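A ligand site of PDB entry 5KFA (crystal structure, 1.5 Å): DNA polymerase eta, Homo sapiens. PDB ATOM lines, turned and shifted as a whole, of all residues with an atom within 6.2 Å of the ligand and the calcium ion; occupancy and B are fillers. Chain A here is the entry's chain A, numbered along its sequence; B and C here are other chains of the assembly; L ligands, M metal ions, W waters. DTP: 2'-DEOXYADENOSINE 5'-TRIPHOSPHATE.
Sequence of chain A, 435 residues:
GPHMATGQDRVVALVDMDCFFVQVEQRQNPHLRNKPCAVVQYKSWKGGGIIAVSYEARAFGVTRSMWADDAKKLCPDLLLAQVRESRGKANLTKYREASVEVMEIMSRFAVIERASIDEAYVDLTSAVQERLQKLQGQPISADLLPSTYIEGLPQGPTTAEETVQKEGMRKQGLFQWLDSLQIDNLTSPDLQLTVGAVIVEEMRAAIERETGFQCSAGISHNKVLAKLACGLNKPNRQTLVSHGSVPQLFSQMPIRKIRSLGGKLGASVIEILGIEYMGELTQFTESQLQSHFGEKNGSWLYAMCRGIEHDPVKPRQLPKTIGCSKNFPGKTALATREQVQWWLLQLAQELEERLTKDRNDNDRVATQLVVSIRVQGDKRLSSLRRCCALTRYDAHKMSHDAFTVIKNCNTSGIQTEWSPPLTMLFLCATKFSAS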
ATOM      1  N   ASP A  16      23.185 -18.890  16.835  1.00  0.00           N
ATOM      2  CA  ASP A  16      23.703 -19.667  15.722  1.00  0.00           C
ATOM      3  C   ASP A  16      23.510 -21.178  15.988  1.00  0.00           C
ATOM      4  O   ASP A  16      24.108 -21.720  16.845  1.00  0.00           O
ATOM      5  CB  ASP A  16      25.173 -19.316  15.581  1.00  0.00           C
ATOM      6  CG  ASP A  16      25.823 -19.780  14.323  1.00  0.00           C
ATOM      7  OD1 ASP A  16      25.292 -20.623  13.686  1.00  0.00           O
ATOM      8  OD2 ASP A  16      26.910 -19.247  14.015  1.00  0.00           O
ATOM      9  N   MET A  17      22.714 -21.822  15.158  1.00  0.00           N
ATOM     10  CA  MET A  17      22.468 -23.249  15.374  1.00  0.00           C
ATOM     11  C   MET A  17      23.758 -24.055  15.212  1.00  0.00           C
ATOM     12  O   MET A  17      24.573 -23.750  14.358  1.00  0.00           O
ATOM     13  CB  MET A  17      21.396 -23.764  14.394  1.00  0.00           C
ATOM     14  CG  MET A  17      20.097 -22.964  14.454  1.00  0.00           C
ATOM     15  SD  MET A  17      19.369 -22.818  16.104  1.00  0.00           S
ATOM     16  CE  MET A  17      19.049 -24.521  16.444  1.00  0.00           C
ATOM     17  N   ASP A  18      23.963 -25.057  16.067  1.00  0.00           N
ATOM     18  CA  ASP A  18      25.165 -25.894  15.905  1.00  0.00           C
ATOM     19  C   ASP A  18      24.995 -26.904  14.788  1.00  0.00           C
ATOM     20  O   ASP A  18      23.964 -27.595  14.727  1.00  0.00           O
ATOM     21  CB  ASP A  18      25.470 -26.682  17.178  1.00  0.00           C
ATOM     22  CG  ASP A  18      25.734 -25.782  18.377  1.00  0.00           C
ATOM     23  OD1 ASP A  18      26.276 -24.678  18.198  1.00  0.00           O
ATOM     24  OD2 ASP A  18      25.406 -26.200  19.484  1.00  0.00           O
ATOM     25  N   CYS A  19      26.013 -26.968  13.928  1.00  0.00           N
ATOM     26  CA  CYS A  19      26.062 -27.902  12.777  1.00  0.00           C
ATOM     27  C   CYS A  19      24.661 -28.181  12.236  1.00  0.00           C
ATOM     28  O   CYS A  19      24.175 -29.322  12.267  1.00  0.00           O
ATOM     29  CB  CYS A  19      26.806 -29.203  13.121  1.00  0.00           C
ATOM     30  SG  CYS A  19      26.267 -30.155  14.541  1.00  0.00           S
ATOM     31  N   PHE A  20      24.014 -27.127  11.753  1.00  0.00           N
ATOM     32  CA  PHE A  20      22.568 -27.122  11.630  1.00  0.00           C
ATOM     33  C   PHE A  20      21.991 -28.232  10.748  1.00  0.00           C
ATOM     34  O   PHE A  20      21.112 -28.969  11.192  1.00  0.00           O
ATOM     35  CB  PHE A  20      22.086 -25.763  11.116  1.00  0.00           C
ATOM     36  CG  PHE A  20      20.586 -25.644  11.066  1.00  0.00           C
ATOM     37  CD1 PHE A  20      19.817 -26.007  12.163  1.00  0.00           C
ATOM     38  CD2 PHE A  20      19.953 -25.173   9.929  1.00  0.00           C
ATOM     39  CE1 PHE A  20      18.423 -25.903  12.122  1.00  0.00           C
ATOM     40  CE2 PHE A  20      18.551 -25.063   9.878  1.00  0.00           C
ATOM     41  CZ  PHE A  20      17.795 -25.422  10.976  1.00  0.00           C
ATOM     42  N   PHE A  21      22.488 -28.393   9.527  1.00  0.00           N
ATOM     43  CA  PHE A  21      21.856 -29.395   8.677  1.00  0.00           C
ATOM     44  C   PHE A  21      22.063 -30.803   9.261  1.00  0.00           C
ATOM     45  O   PHE A  21      21.213 -31.674   9.084  1.00  0.00           O
ATOM     46  CB  PHE A  21      22.399 -29.380   7.241  1.00  0.00           C
ATOM     47  CG  PHE A  21      21.976 -28.191   6.427  1.00  0.00           C
ATOM     48  CD1 PHE A  21      21.423 -27.046   6.999  1.00  0.00           C
ATOM     49  CD2 PHE A  21      22.140 -28.224   5.051  1.00  0.00           C
ATOM     50  CE1 PHE A  21      21.042 -25.964   6.202  1.00  0.00           C
ATOM     51  CE2 PHE A  21      21.769 -27.145   4.245  1.00  0.00           C
ATOM     52  CZ  PHE A  21      21.218 -26.016   4.836  1.00  0.00           C
ATOM     53  N   VAL A  22      23.197 -31.034   9.921  1.00  0.00           N
ATOM     54  CA  VAL A  22      23.444 -32.303  10.591  1.00  0.00           C
ATOM     55  C   VAL A  22      22.409 -32.525  11.681  1.00  0.00           C
ATOM     56  O   VAL A  22      21.851 -33.622  11.789  1.00  0.00           O
ATOM     57  CB  VAL A  22      24.862 -32.350  11.171  1.00  0.00           C
ATOM     58  CG1 VAL A  22      25.012 -33.471  12.204  1.00  0.00           C
ATOM     59  CG2 VAL A  22      25.878 -32.506  10.042  1.00  0.00           C
ATOM     60  N   GLN A  41      25.775 -33.294  -0.613  1.00  0.00           N
ATOM     61  CA  GLN A  41      24.853 -33.101  -1.729  1.00  0.00           C
ATOM     62  C   GLN A  41      25.408 -33.805  -2.943  1.00  0.00           C
ATOM     63  O   GLN A  41      26.613 -33.726  -3.221  1.00  0.00           O
ATOM     64  CB  GLN A  41      24.591 -31.619  -2.011  1.00  0.00           C
ATOM     65  CG  GLN A  41      25.813 -30.752  -2.100  1.00  0.00           C
ATOM     66  CD  GLN A  41      25.472 -29.275  -2.078  1.00  0.00           C
ATOM     67  OE1 GLN A  41      24.328 -28.889  -1.822  1.00  0.00           O
ATOM     68  NE2 GLN A  41      26.467 -28.439  -2.363  1.00  0.00           N
ATOM     69  N   ILE A  51      28.497 -30.406   3.077  1.00  0.00           N
ATOM     70  CA  ILE A  51      28.084 -29.045   3.406  1.00  0.00           C
ATOM     71  C   ILE A  51      27.852 -28.815   4.901  1.00  0.00           C
ATOM     72  O   ILE A  51      27.717 -27.666   5.302  1.00  0.00           O
ATOM     73  CB  ILE A  51      26.824 -28.622   2.626  1.00  0.00           C
ATOM     74  CG1 ILE A  51      25.630 -29.542   2.915  1.00  0.00           C
ATOM     75  CG2 ILE A  51      27.128 -28.567   1.119  1.00  0.00           C
ATOM     76  CD1 ILE A  51      24.305 -29.034   2.306  1.00  0.00           C
ATOM     77  N   ALA A  52      27.834 -29.869   5.710  1.00  0.00           N
ATOM     78  CA  ALA A  52      27.722 -29.715   7.171  1.00  0.00           C
ATOM     79  C   ALA A  52      28.350 -30.901   7.863  1.00  0.00           C
ATOM     80  O   ALA A  52      28.299 -32.007   7.326  1.00  0.00           O
ATOM     81  CB  ALA A  52      26.256 -29.549   7.601  1.00  0.00           C
ATOM     82  N   VAL A  53      28.949 -30.687   9.046  1.00  0.00           N
ATOM     83  CA  VAL A  53      29.778 -31.686   9.722  1.00  0.00           C
ATOM     84  C   VAL A  53      29.527 -31.689  11.228  1.00  0.00           C
ATOM     85  O   VAL A  53      29.611 -30.638  11.866  1.00  0.00           O
ATOM     86  CB  VAL A  53      31.297 -31.420   9.489  1.00  0.00           C
ATOM     87  CG1 VAL A  53      32.126 -32.575  10.032  1.00  0.00           C
ATOM     88  CG2 VAL A  53      31.607 -31.211   8.013  1.00  0.00           C
ATOM     89  N   TYR A  55      30.234 -32.326  15.232  1.00  0.00           N
ATOM     90  CA  TYR A  55      31.444 -32.035  15.987  1.00  0.00           C
ATOM     91  C   TYR A  55      32.274 -33.300  16.211  1.00  0.00           C
ATOM     92  O   TYR A  55      33.506 -33.227  16.228  1.00  0.00           O
ATOM     93  CB  TYR A  55      31.092 -31.332  17.303  1.00  0.00           C
ATOM     94  CG  TYR A  55      30.809 -29.864  17.037  1.00  0.00           C
ATOM     95  CD1 TYR A  55      29.572 -29.454  16.531  1.00  0.00           C
ATOM     96  CD2 TYR A  55      31.806 -28.900  17.195  1.00  0.00           C
ATOM     97  CE1 TYR A  55      29.329 -28.121  16.239  1.00  0.00           C
ATOM     98  CE2 TYR A  55      31.571 -27.572  16.914  1.00  0.00           C
ATOM     99  CZ  TYR A  55      30.344 -27.182  16.427  1.00  0.00           C
ATOM    100  OH  TYR A  55      30.127 -25.843  16.149  1.00  0.00           O
ATOM    101  N   ARG A  58      34.262 -33.496  13.069  1.00  0.00           N
ATOM    102  CA  ARG A  58      35.295 -32.452  12.985  1.00  0.00           C
ATOM    103  C   ARG A  58      36.578 -32.860  13.728  1.00  0.00           C
ATOM    104  O   ARG A  58      37.674 -32.439  13.343  1.00  0.00           O
ATOM    105  CB  ARG A  58      34.792 -31.125  13.534  1.00  0.00           C
ATOM    106  CG  ARG A  58      33.599 -30.583  12.789  1.00  0.00           C
ATOM    107  CD  ARG A  58      33.118 -29.273  13.379  1.00  0.00           C
ATOM    108  NE  ARG A  58      31.779 -28.980  12.885  1.00  0.00           N
ATOM    109  CZ  ARG A  58      31.188 -27.794  12.931  1.00  0.00           C
ATOM    110  NH1 ARG A  58      31.803 -26.754  13.470  1.00  0.00           N
ATOM    111  NH2 ARG A  58      29.952 -27.663  12.435  1.00  0.00           N
ATOM    112  N   ARG A  64      33.642 -28.807   5.788  1.00  0.00           N
ATOM    113  CA  ARG A  64      32.840 -28.367   4.652  1.00  0.00           C
ATOM    114  C   ARG A  64      33.726 -28.259   3.397  1.00  0.00           C
ATOM    115  O   ARG A  64      34.919 -27.981   3.516  1.00  0.00           O
ATOM    116  CB  ARG A  64      32.154 -27.037   4.991  1.00  0.00           C
ATOM    117  CG  ARG A  64      31.450 -26.328   3.844  1.00  0.00           C
ATOM    118  CD  ARG A  64      30.663 -25.136   4.365  1.00  0.00           C
ATOM    119  NE  ARG A  64      29.687 -25.565   5.366  1.00  0.00           N
ATOM    120  CZ  ARG A  64      29.543 -25.012   6.570  1.00  0.00           C
ATOM    121  NH1 ARG A  64      30.287 -23.966   6.930  1.00  0.00           N
ATOM    122  NH2 ARG A  64      28.628 -25.492   7.412  1.00  0.00           N
ATOM    123  N   SER A 116      20.741 -15.581   8.367  1.00  0.00           N
ATOM    124  CA  SER A 116      21.015 -16.699   7.468  1.00  0.00           C
ATOM    125  C   SER A 116      20.021 -17.792   7.764  1.00  0.00           C
ATOM    126  O   SER A 116      19.155 -17.627   8.607  1.00  0.00           O
ATOM    127  CB  SER A 116      22.434 -17.227   7.641  1.00  0.00           C
ATOM    128  OG  SER A 116      22.545 -17.956   8.859  1.00  0.00           O
ATOM    129  N   ILE A 117      20.188 -18.951   7.124  1.00  0.00           N
ATOM    130  CA  ILE A 117      19.271 -20.057   7.356  1.00  0.00           C
ATOM    131  C   ILE A 117      19.288 -20.521   8.826  1.00  0.00           C
ATOM    132  O   ILE A 117      18.321 -21.108   9.302  1.00  0.00           O
ATOM    133  CB  ILE A 117      19.592 -21.240   6.407  1.00  0.00           C
ATOM    134  CG1 ILE A 117      18.418 -22.221   6.351  1.00  0.00           C
ATOM    135  CG2 ILE A 117      20.889 -21.916   6.820  1.00  0.00           C
ATOM    136  CD1 ILE A 117      18.472 -23.150   5.141  1.00  0.00           C
ATOM    137  N   ASP A 118      20.368 -20.258   9.566  1.00  0.00           N
ATOM    138  CA  ASP A 118      20.410 -20.769  10.934  1.00  0.00           C
ATOM    139  C   ASP A 118      20.963 -19.768  11.958  1.00  0.00           C
ATOM    140  O   ASP A 118      21.389 -20.162  13.050  1.00  0.00           O
ATOM    141  CB  ASP A 118      21.224 -22.059  10.973  1.00  0.00           C
ATOM    142  CG  ASP A 118      22.720 -21.805  11.019  1.00  0.00           C
ATOM    143  OD1 ASP A 118      23.420 -22.590  11.687  1.00  0.00           O
ATOM    144  OD2 ASP A 118      23.188 -20.792  10.433  1.00  0.00           O
ATOM    145  N   GLU A 119      20.922 -18.487  11.632  1.00  0.00           N
ATOM    146  CA  GLU A 119      21.425 -17.427  12.504  1.00  0.00           C
ATOM    147  C   GLU A 119      20.421 -16.312  12.595  1.00  0.00           C
ATOM    148  O   GLU A 119      19.873 -15.935  11.640  1.00  0.00           O
ATOM    149  CB  GLU A 119      22.715 -16.806  11.961  1.00  0.00           C
ATOM    150  CG  GLU A 119      23.925 -17.742  11.903  1.00  0.00           C
ATOM    151  CD  GLU A 119      25.200 -17.068  11.554  1.00  0.00           C
ATOM    152  OE1 GLU A 119      25.197 -15.887  11.386  1.00  0.00           O
ATOM    153  OE2 GLU A 119      26.205 -17.731  11.546  1.00  0.00           O
ATOM    154  N   LYS A 227      28.225 -11.561  17.306  1.00  0.00           N
ATOM    155  CA  LYS A 227      28.653 -12.599  16.367  1.00  0.00           C
ATOM    156  C   LYS A 227      30.020 -13.173  16.764  1.00  0.00           C
ATOM    157  O   LYS A 227      30.205 -14.394  16.796  1.00  0.00           O
ATOM    158  CB  LYS A 227      28.704 -12.052  14.941  1.00  0.00           C
ATOM    159  CG  LYS A 227      29.251 -13.030  13.917  1.00  0.00           C
ATOM    160  CD  LYS A 227      28.428 -14.303  13.855  1.00  0.00           C
ATOM    161  CE  LYS A 227      28.951 -15.249  12.782  1.00  0.00           C
ATOM    162  NZ  LYS A 227      28.279 -16.568  12.862  1.00  0.00           N
ATOM    163  N   LYS A 234      31.813 -22.814  21.168  1.00  0.00           N
ATOM    164  CA  LYS A 234      30.881 -23.683  20.429  1.00  0.00           C
ATOM    165  C   LYS A 234      31.313 -25.111  20.712  1.00  0.00           C
ATOM    166  O   LYS A 234      32.504 -25.366  20.943  1.00  0.00           O
ATOM    167  CB  LYS A 234      30.907 -23.388  18.921  1.00  0.00           C
ATOM    168  CG  LYS A 234      29.862 -22.389  18.385  1.00  0.00           C
ATOM    169  CD  LYS A 234      29.625 -22.592  16.856  1.00  0.00           C
ATOM    170  CE  LYS A 234      28.382 -21.858  16.292  1.00  0.00           C
ATOM    171  NZ  LYS A 234      27.069 -22.647  16.347  1.00  0.00           N
ATOM    172  N   PRO A 235      30.374 -26.058  20.712  1.00  0.00           N
ATOM    173  CA  PRO A 235      28.937 -25.885  20.501  1.00  0.00           C
ATOM    174  C   PRO A 235      28.185 -25.835  21.821  1.00  0.00           C
ATOM    175  O   PRO A 235      28.774 -26.029  22.893  1.00  0.00           O
ATOM    176  CB  PRO A 235      28.557 -27.144  19.729  1.00  0.00           C
ATOM    177  CG  PRO A 235      29.450 -28.197  20.366  1.00  0.00           C
ATOM    178  CD  PRO A 235      30.745 -27.477  20.738  1.00  0.00           C
ATOM    179  P    DT B   3      36.834 -28.162  -7.188  1.00  0.00           P
ATOM    180  OP1  DT B   3      37.923 -27.706  -8.085  1.00  0.00           O
ATOM    181  OP2  DT B   3      37.144 -28.924  -5.963  1.00  0.00           O
ATOM    182  O5'  DT B   3      35.982 -26.873  -6.787  1.00  0.00           O
ATOM    183  C5'  DT B   3      35.195 -26.877  -5.606  1.00  0.00           C
ATOM    184  C4'  DT B   3      33.904 -27.655  -5.820  1.00  0.00           C
ATOM    185  O4'  DT B   3      33.330 -27.979  -4.530  1.00  0.00           O
ATOM    186  C3'  DT B   3      32.824 -26.897  -6.578  1.00  0.00           C
ATOM    187  O3'  DT B   3      32.031 -27.824  -7.298  1.00  0.00           O
ATOM    188  C2'  DT B   3      32.037 -26.245  -5.461  1.00  0.00           C
ATOM    189  C1'  DT B   3      32.077 -27.331  -4.387  1.00  0.00           C
ATOM    190  N1   DT B   3      31.977 -26.804  -2.999  1.00  0.00           N
ATOM    191  C2   DT B   3      31.052 -27.338  -2.131  1.00  0.00           C
ATOM    192  O2   DT B   3      30.293 -28.245  -2.433  1.00  0.00           O
ATOM    193  N3   DT B   3      31.056 -26.784  -0.872  1.00  0.00           N
ATOM    194  C4   DT B   3      31.876 -25.758  -0.415  1.00  0.00           C
ATOM    195  O4   DT B   3      31.811 -25.334   0.727  1.00  0.00           O
ATOM    196  C5   DT B   3      32.826 -25.248  -1.383  1.00  0.00           C
ATOM    197  C7   DT B   3      33.766 -24.141  -1.008  1.00  0.00           C
ATOM    198  C6   DT B   3      32.838 -25.792  -2.609  1.00  0.00           C
ATOM    199  P    DT B   4      30.750 -27.324  -8.135  1.00  0.00           P
ATOM    200  OP1  DT B   4      30.377 -28.405  -9.065  1.00  0.00           O
ATOM    201  OP2  DT B   4      31.033 -25.961  -8.644  1.00  0.00           O
ATOM    202  O5'  DT B   4      29.609 -27.187  -7.029  1.00  0.00           O
ATOM    203  C5'  DT B   4      29.034 -28.330  -6.483  1.00  0.00           C
ATOM    204  C4'  DT B   4      27.726 -27.985  -5.802  1.00  0.00           C
ATOM    205  O4'  DT B   4      27.995 -27.351  -4.541  1.00  0.00           O
ATOM    206  C3'  DT B   4      26.831 -27.030  -6.578  1.00  0.00           C
ATOM    207  O3'  DT B   4      25.504 -27.468  -6.389  1.00  0.00           O
ATOM    208  C2'  DT B   4      27.080 -25.685  -5.893  1.00  0.00           C
ATOM    209  C1'  DT B   4      27.268 -26.138  -4.456  1.00  0.00           C
ATOM    210  N1   DT B   4      28.041 -25.230  -3.589  1.00  0.00           N
ATOM    211  C2   DT B   4      27.640 -25.134  -2.292  1.00  0.00           C
ATOM    212  O2   DT B   4      26.664 -25.722  -1.857  1.00  0.00           O
ATOM    213  N3   DT B   4      28.416 -24.332  -1.513  1.00  0.00           N
ATOM    214  C4   DT B   4      29.523 -23.630  -1.876  1.00  0.00           C
ATOM    215  O4   DT B   4      30.146 -22.929  -1.079  1.00  0.00           O
ATOM    216  C5   DT B   4      29.920 -23.782  -3.268  1.00  0.00           C
ATOM    217  C7   DT B   4      31.131 -23.059  -3.802  1.00  0.00           C
ATOM    218  C6   DT B   4      29.167 -24.585  -4.045  1.00  0.00           C
ATOM    219  P    DA B   5      24.263 -26.721  -7.073  1.00  0.00           P
ATOM    220  OP1  DA B   5      23.346 -27.775  -7.511  1.00  0.00           O
ATOM    221  OP2  DA B   5      24.754 -25.729  -8.051  1.00  0.00           O
ATOM    222  O5'  DA B   5      23.601 -25.944  -5.864  1.00  0.00           O
ATOM    223  C5'  DA B   5      22.960 -26.650  -4.819  1.00  0.00           C
ATOM    224  C4'  DA B   5      22.354 -25.679  -3.833  1.00  0.00           C
ATOM    225  O4'  DA B   5      23.409 -24.997  -3.095  1.00  0.00           O
ATOM    226  C3'  DA B   5      21.498 -24.579  -4.463  1.00  0.00           C
ATOM    227  O3'  DA B   5      20.350 -24.344  -3.644  1.00  0.00           O
ATOM    228  C2'  DA B   5      22.435 -23.376  -4.466  1.00  0.00           C
ATOM    229  C1'  DA B   5      23.156 -23.596  -3.141  1.00  0.00           C
ATOM    230  N9   DA B   5      24.410 -22.891  -3.016  1.00  0.00           N
ATOM    231  C8   DA B   5      25.323 -22.648  -3.996  1.00  0.00           C
ATOM    232  N7   DA B   5      26.385 -21.987  -3.571  1.00  0.00           N
ATOM    233  C5   DA B   5      26.146 -21.804  -2.222  1.00  0.00           C
ATOM    234  C6   DA B   5      26.888 -21.176  -1.196  1.00  0.00           C
ATOM    235  N6   DA B   5      28.071 -20.607  -1.401  1.00  0.00           N
ATOM    236  N1   DA B   5      26.357 -21.171   0.041  1.00  0.00           N
ATOM    237  C2   DA B   5      25.169 -21.748   0.244  1.00  0.00           C
ATOM    238  N3   DA B   5      24.386 -22.372  -0.634  1.00  0.00           N
ATOM    239  C4   DA B   5      24.940 -22.356  -1.857  1.00  0.00           C
ATOM    240  P    DT C   8      29.817 -16.693   7.999  1.00  0.00           P
ATOM    241  OP1  DT C   8      29.906 -16.631   9.473  1.00  0.00           O
ATOM    242  OP2  DT C   8      30.864 -17.437   7.264  1.00  0.00           O
ATOM    243  O5'  DT C   8      28.383 -17.285   7.512  1.00  0.00           O
ATOM    244  C5'  DT C   8      27.233 -17.212   8.350  1.00  0.00           C
ATOM    245  C4'  DT C   8      26.020 -17.914   7.736  1.00  0.00           C
ATOM    246  O4'  DT C   8      26.068 -17.836   6.286  1.00  0.00           O
ATOM    247  C3'  DT C   8      25.843 -19.387   8.097  1.00  0.00           C
ATOM    248  O3'  DT C   8      24.479 -19.641   8.366  1.00  0.00           O
ATOM    249  C2'  DT C   8      26.307 -20.114   6.831  1.00  0.00           C
ATOM    250  C1'  DT C   8      25.931 -19.133   5.726  1.00  0.00           C
ATOM    251  N1   DT C   8      26.805 -19.243   4.505  1.00  0.00           N
ATOM    252  C2   DT C   8      26.311 -19.872   3.383  1.00  0.00           C
ATOM    253  O2   DT C   8      25.196 -20.366   3.338  1.00  0.00           O
ATOM    254  N3   DT C   8      27.178 -19.917   2.328  1.00  0.00           N
ATOM    255  C4   DT C   8      28.464 -19.415   2.280  1.00  0.00           C
ATOM    256  O4   DT C   8      29.171 -19.493   1.276  1.00  0.00           O
ATOM    257  C5   DT C   8      28.920 -18.764   3.480  1.00  0.00           C
ATOM    258  C7   DT C   8      30.296 -18.176   3.538  1.00  0.00           C
ATOM    259  C6   DT C   8      28.076 -18.719   4.528  1.00  0.00           C
HETATM  260  PG  DTP L   1      28.546 -24.488  13.228  1.00  0.00           P
HETATM  261  O1G DTP L   1      27.743 -23.201  13.170  1.00  0.00           O
HETATM  262  O2G DTP L   1      28.184 -25.295  14.444  1.00  0.00           O
HETATM  263  O3G DTP L   1      30.041 -24.250  13.132  1.00  0.00           O
HETATM  264  PB  DTP L   1      27.111 -25.113  10.835  1.00  0.00           P
HETATM  265  O1B DTP L   1      25.792 -24.673  11.451  1.00  0.00           O
HETATM  266  O2B DTP L   1      26.947 -26.346   9.985  1.00  0.00           O
HETATM  267  O3B DTP L   1      28.201 -25.415  11.969  1.00  0.00           O
HETATM  268  PA  DTP L   1      27.135 -22.586   9.436  1.00  0.00           P
HETATM  269  O1A DTP L   1      26.555 -21.812  10.583  1.00  0.00           O
HETATM  270  O2A DTP L   1      28.266 -21.877   8.733  1.00  0.00           O
HETATM  271  O3A DTP L   1      27.752 -23.972   9.922  1.00  0.00           O
HETATM  272  O5' DTP L   1      26.048 -22.916   8.348  1.00  0.00           O
HETATM  273  C5' DTP L   1      24.727 -23.293   8.663  1.00  0.00           C
HETATM  274  C4' DTP L   1      24.214 -24.268   7.616  1.00  0.00           C
HETATM  275  O4' DTP L   1      24.228 -23.607   6.365  1.00  0.00           O
HETATM  276  C3' DTP L   1      25.080 -25.426   7.478  1.00  0.00           C
HETATM  277  O3' DTP L   1      24.672 -26.487   8.358  1.00  0.00           O
HETATM  278  C2' DTP L   1      24.964 -25.829   6.077  1.00  0.00           C
HETATM  279  C1' DTP L   1      24.712 -24.531   5.379  1.00  0.00           C
HETATM  280  N9  DTP L   1      25.894 -24.004   4.779  1.00  0.00           N
HETATM  281  C8  DTP L   1      26.861 -23.251   5.362  1.00  0.00           C
HETATM  282  N7  DTP L   1      27.804 -22.945   4.480  1.00  0.00           N
HETATM  283  C5  DTP L   1      27.479 -23.488   3.291  1.00  0.00           C
HETATM  284  C6  DTP L   1      28.052 -23.524   2.025  1.00  0.00           C
HETATM  285  N6  DTP L   1      29.295 -22.856   1.773  1.00  0.00           N
HETATM  286  N1  DTP L   1      27.442 -24.199   1.050  1.00  0.00           N
HETATM  287  C2  DTP L   1      26.266 -24.838   1.230  1.00  0.00           C
HETATM  288  N3  DTP L   1      25.673 -24.820   2.462  1.00  0.00           N
HETATM  289  C4  DTP L   1      26.256 -24.170   3.473  1.00  0.00           C
HETATM  290 CA    CA M   1      25.578 -22.684  12.599  1.00  0.00          CA
HETATM  291  O   HOH W   1      23.045 -25.218   1.790  1.00  0.00           O
HETATM  292  O   HOH W   2      28.274 -19.976  11.751  1.00  0.00           O
HETATM  293  O   HOH W   3      29.125 -27.972   9.661  1.00  0.00           O
HETATM  294  O   HOH W   4      31.547 -24.288  10.901  1.00  0.00           O
HETATM  295  O   HOH W   5      30.468 -21.391  12.865  1.00  0.00           O
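The side-chain hydroxyl (OH) of Tyr 55 sits at hydrogen-bond distance from an oxygen (O2G) of the ligand (2.6 Å).
O4 of DT 4 of chain B lies within hydrogen-bond range of a nitrogen (N6) of the ligand (3.0 Å).
The backbone NH (N) of Cys 19 sits at hydrogen-bond distance from an oxygen (O2G) of the ligand, 2.8 Å away.
The guanidinium group (NH1) of Arg 58 lies within salt-bridge range of an oxygen (O3G) of the ligand, at 3.1 Å.
The backbone NH of Phe 20 lies close to an oxygen (O1B) of the ligand.
O2B of the ligand is in salt-bridge range of NH2 of Arg 64.
An oxygen (O3') of the ligand is in hydrogen-bond range of the backbone NH (N) of Phe 21.
A nitrogen (N6) of the ligand sits at hydrogen-bond distance from O4 of DT 8 of chain C (3.4 Å).
O2G of the ligand is in salt-bridge range of NZ of Lys 234, at 3.4 Å.
The backbone NH of Asp 118 lies close to the side-chain hydroxyl of Ser 116.
The side-chain amino group (NZ) of Lys 234 sits at hydrogen-bond distance from the backbone carbonyl oxygen (O) of Asp 16.
The side-chain carboxylate of Asp 16 lies within salt-bridge range of the side-chain amino group of Lys 227, 3.2 Å away.
The side-chain hydroxyl of Tyr 55 lies within hydrogen-bond range of the guanidinium group of Arg 58, 3.3 Å away.
O2 of DT 4 of chain B sits at hydrogen-bond distance from NE2 of Gln 41, at 2.8 Å.
NE of Arg 58 sits at hydrogen-bond distance from O of Val 53 (2.9 Å).
OP1 of DT 8 of chain C lies within salt-bridge range of the side-chain amino group (NZ) of Lys 227, 3.8 Å away.
The side-chain carboxylate (OD1) of Asp 18 lies within salt-bridge range of the side-chain amino group (NZ) of Lys 234 (2.9 Å).
N1 of DA 5 of chain B lies close to a nitrogen (N1) of the ligand (3.4 Å).
Asp 18 touches the ligand (CA to O2G, 3.4 Å).
Ile 51 touches the ligand (O to C2', 3.4 Å).
Ala 52 touches the ligand.
Ile 117 touches the ligand.
DT 3 of chain B touches the ligand.
Hydrophobic or aromatic side chains within 4 Å of the ligand: Phe 20, Phe 21, Ile 51, Ala 52, Tyr 55 and Ile 117.
Of the 25 residues printed, 18 come within 4 Å of the ligand.
The nearest printed residue that does not touch the ligand is Glu 119 (4.2 Å).
Three residues have an atom within 4 Å of the calcium ion: Asp 16, Met 17 and Asp 118.
The calcium ion is bound by O of Met 17, O1G of the ligand, O1B of the ligand, OD1 of Asp 118, OD1 of Asp 16 and O1A of the ligand.
Water W2 lies within hydrogen-bond range of OD2 of Asp 16 (2.7 Å) and OE2 of Glu 119 (3.1 Å).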
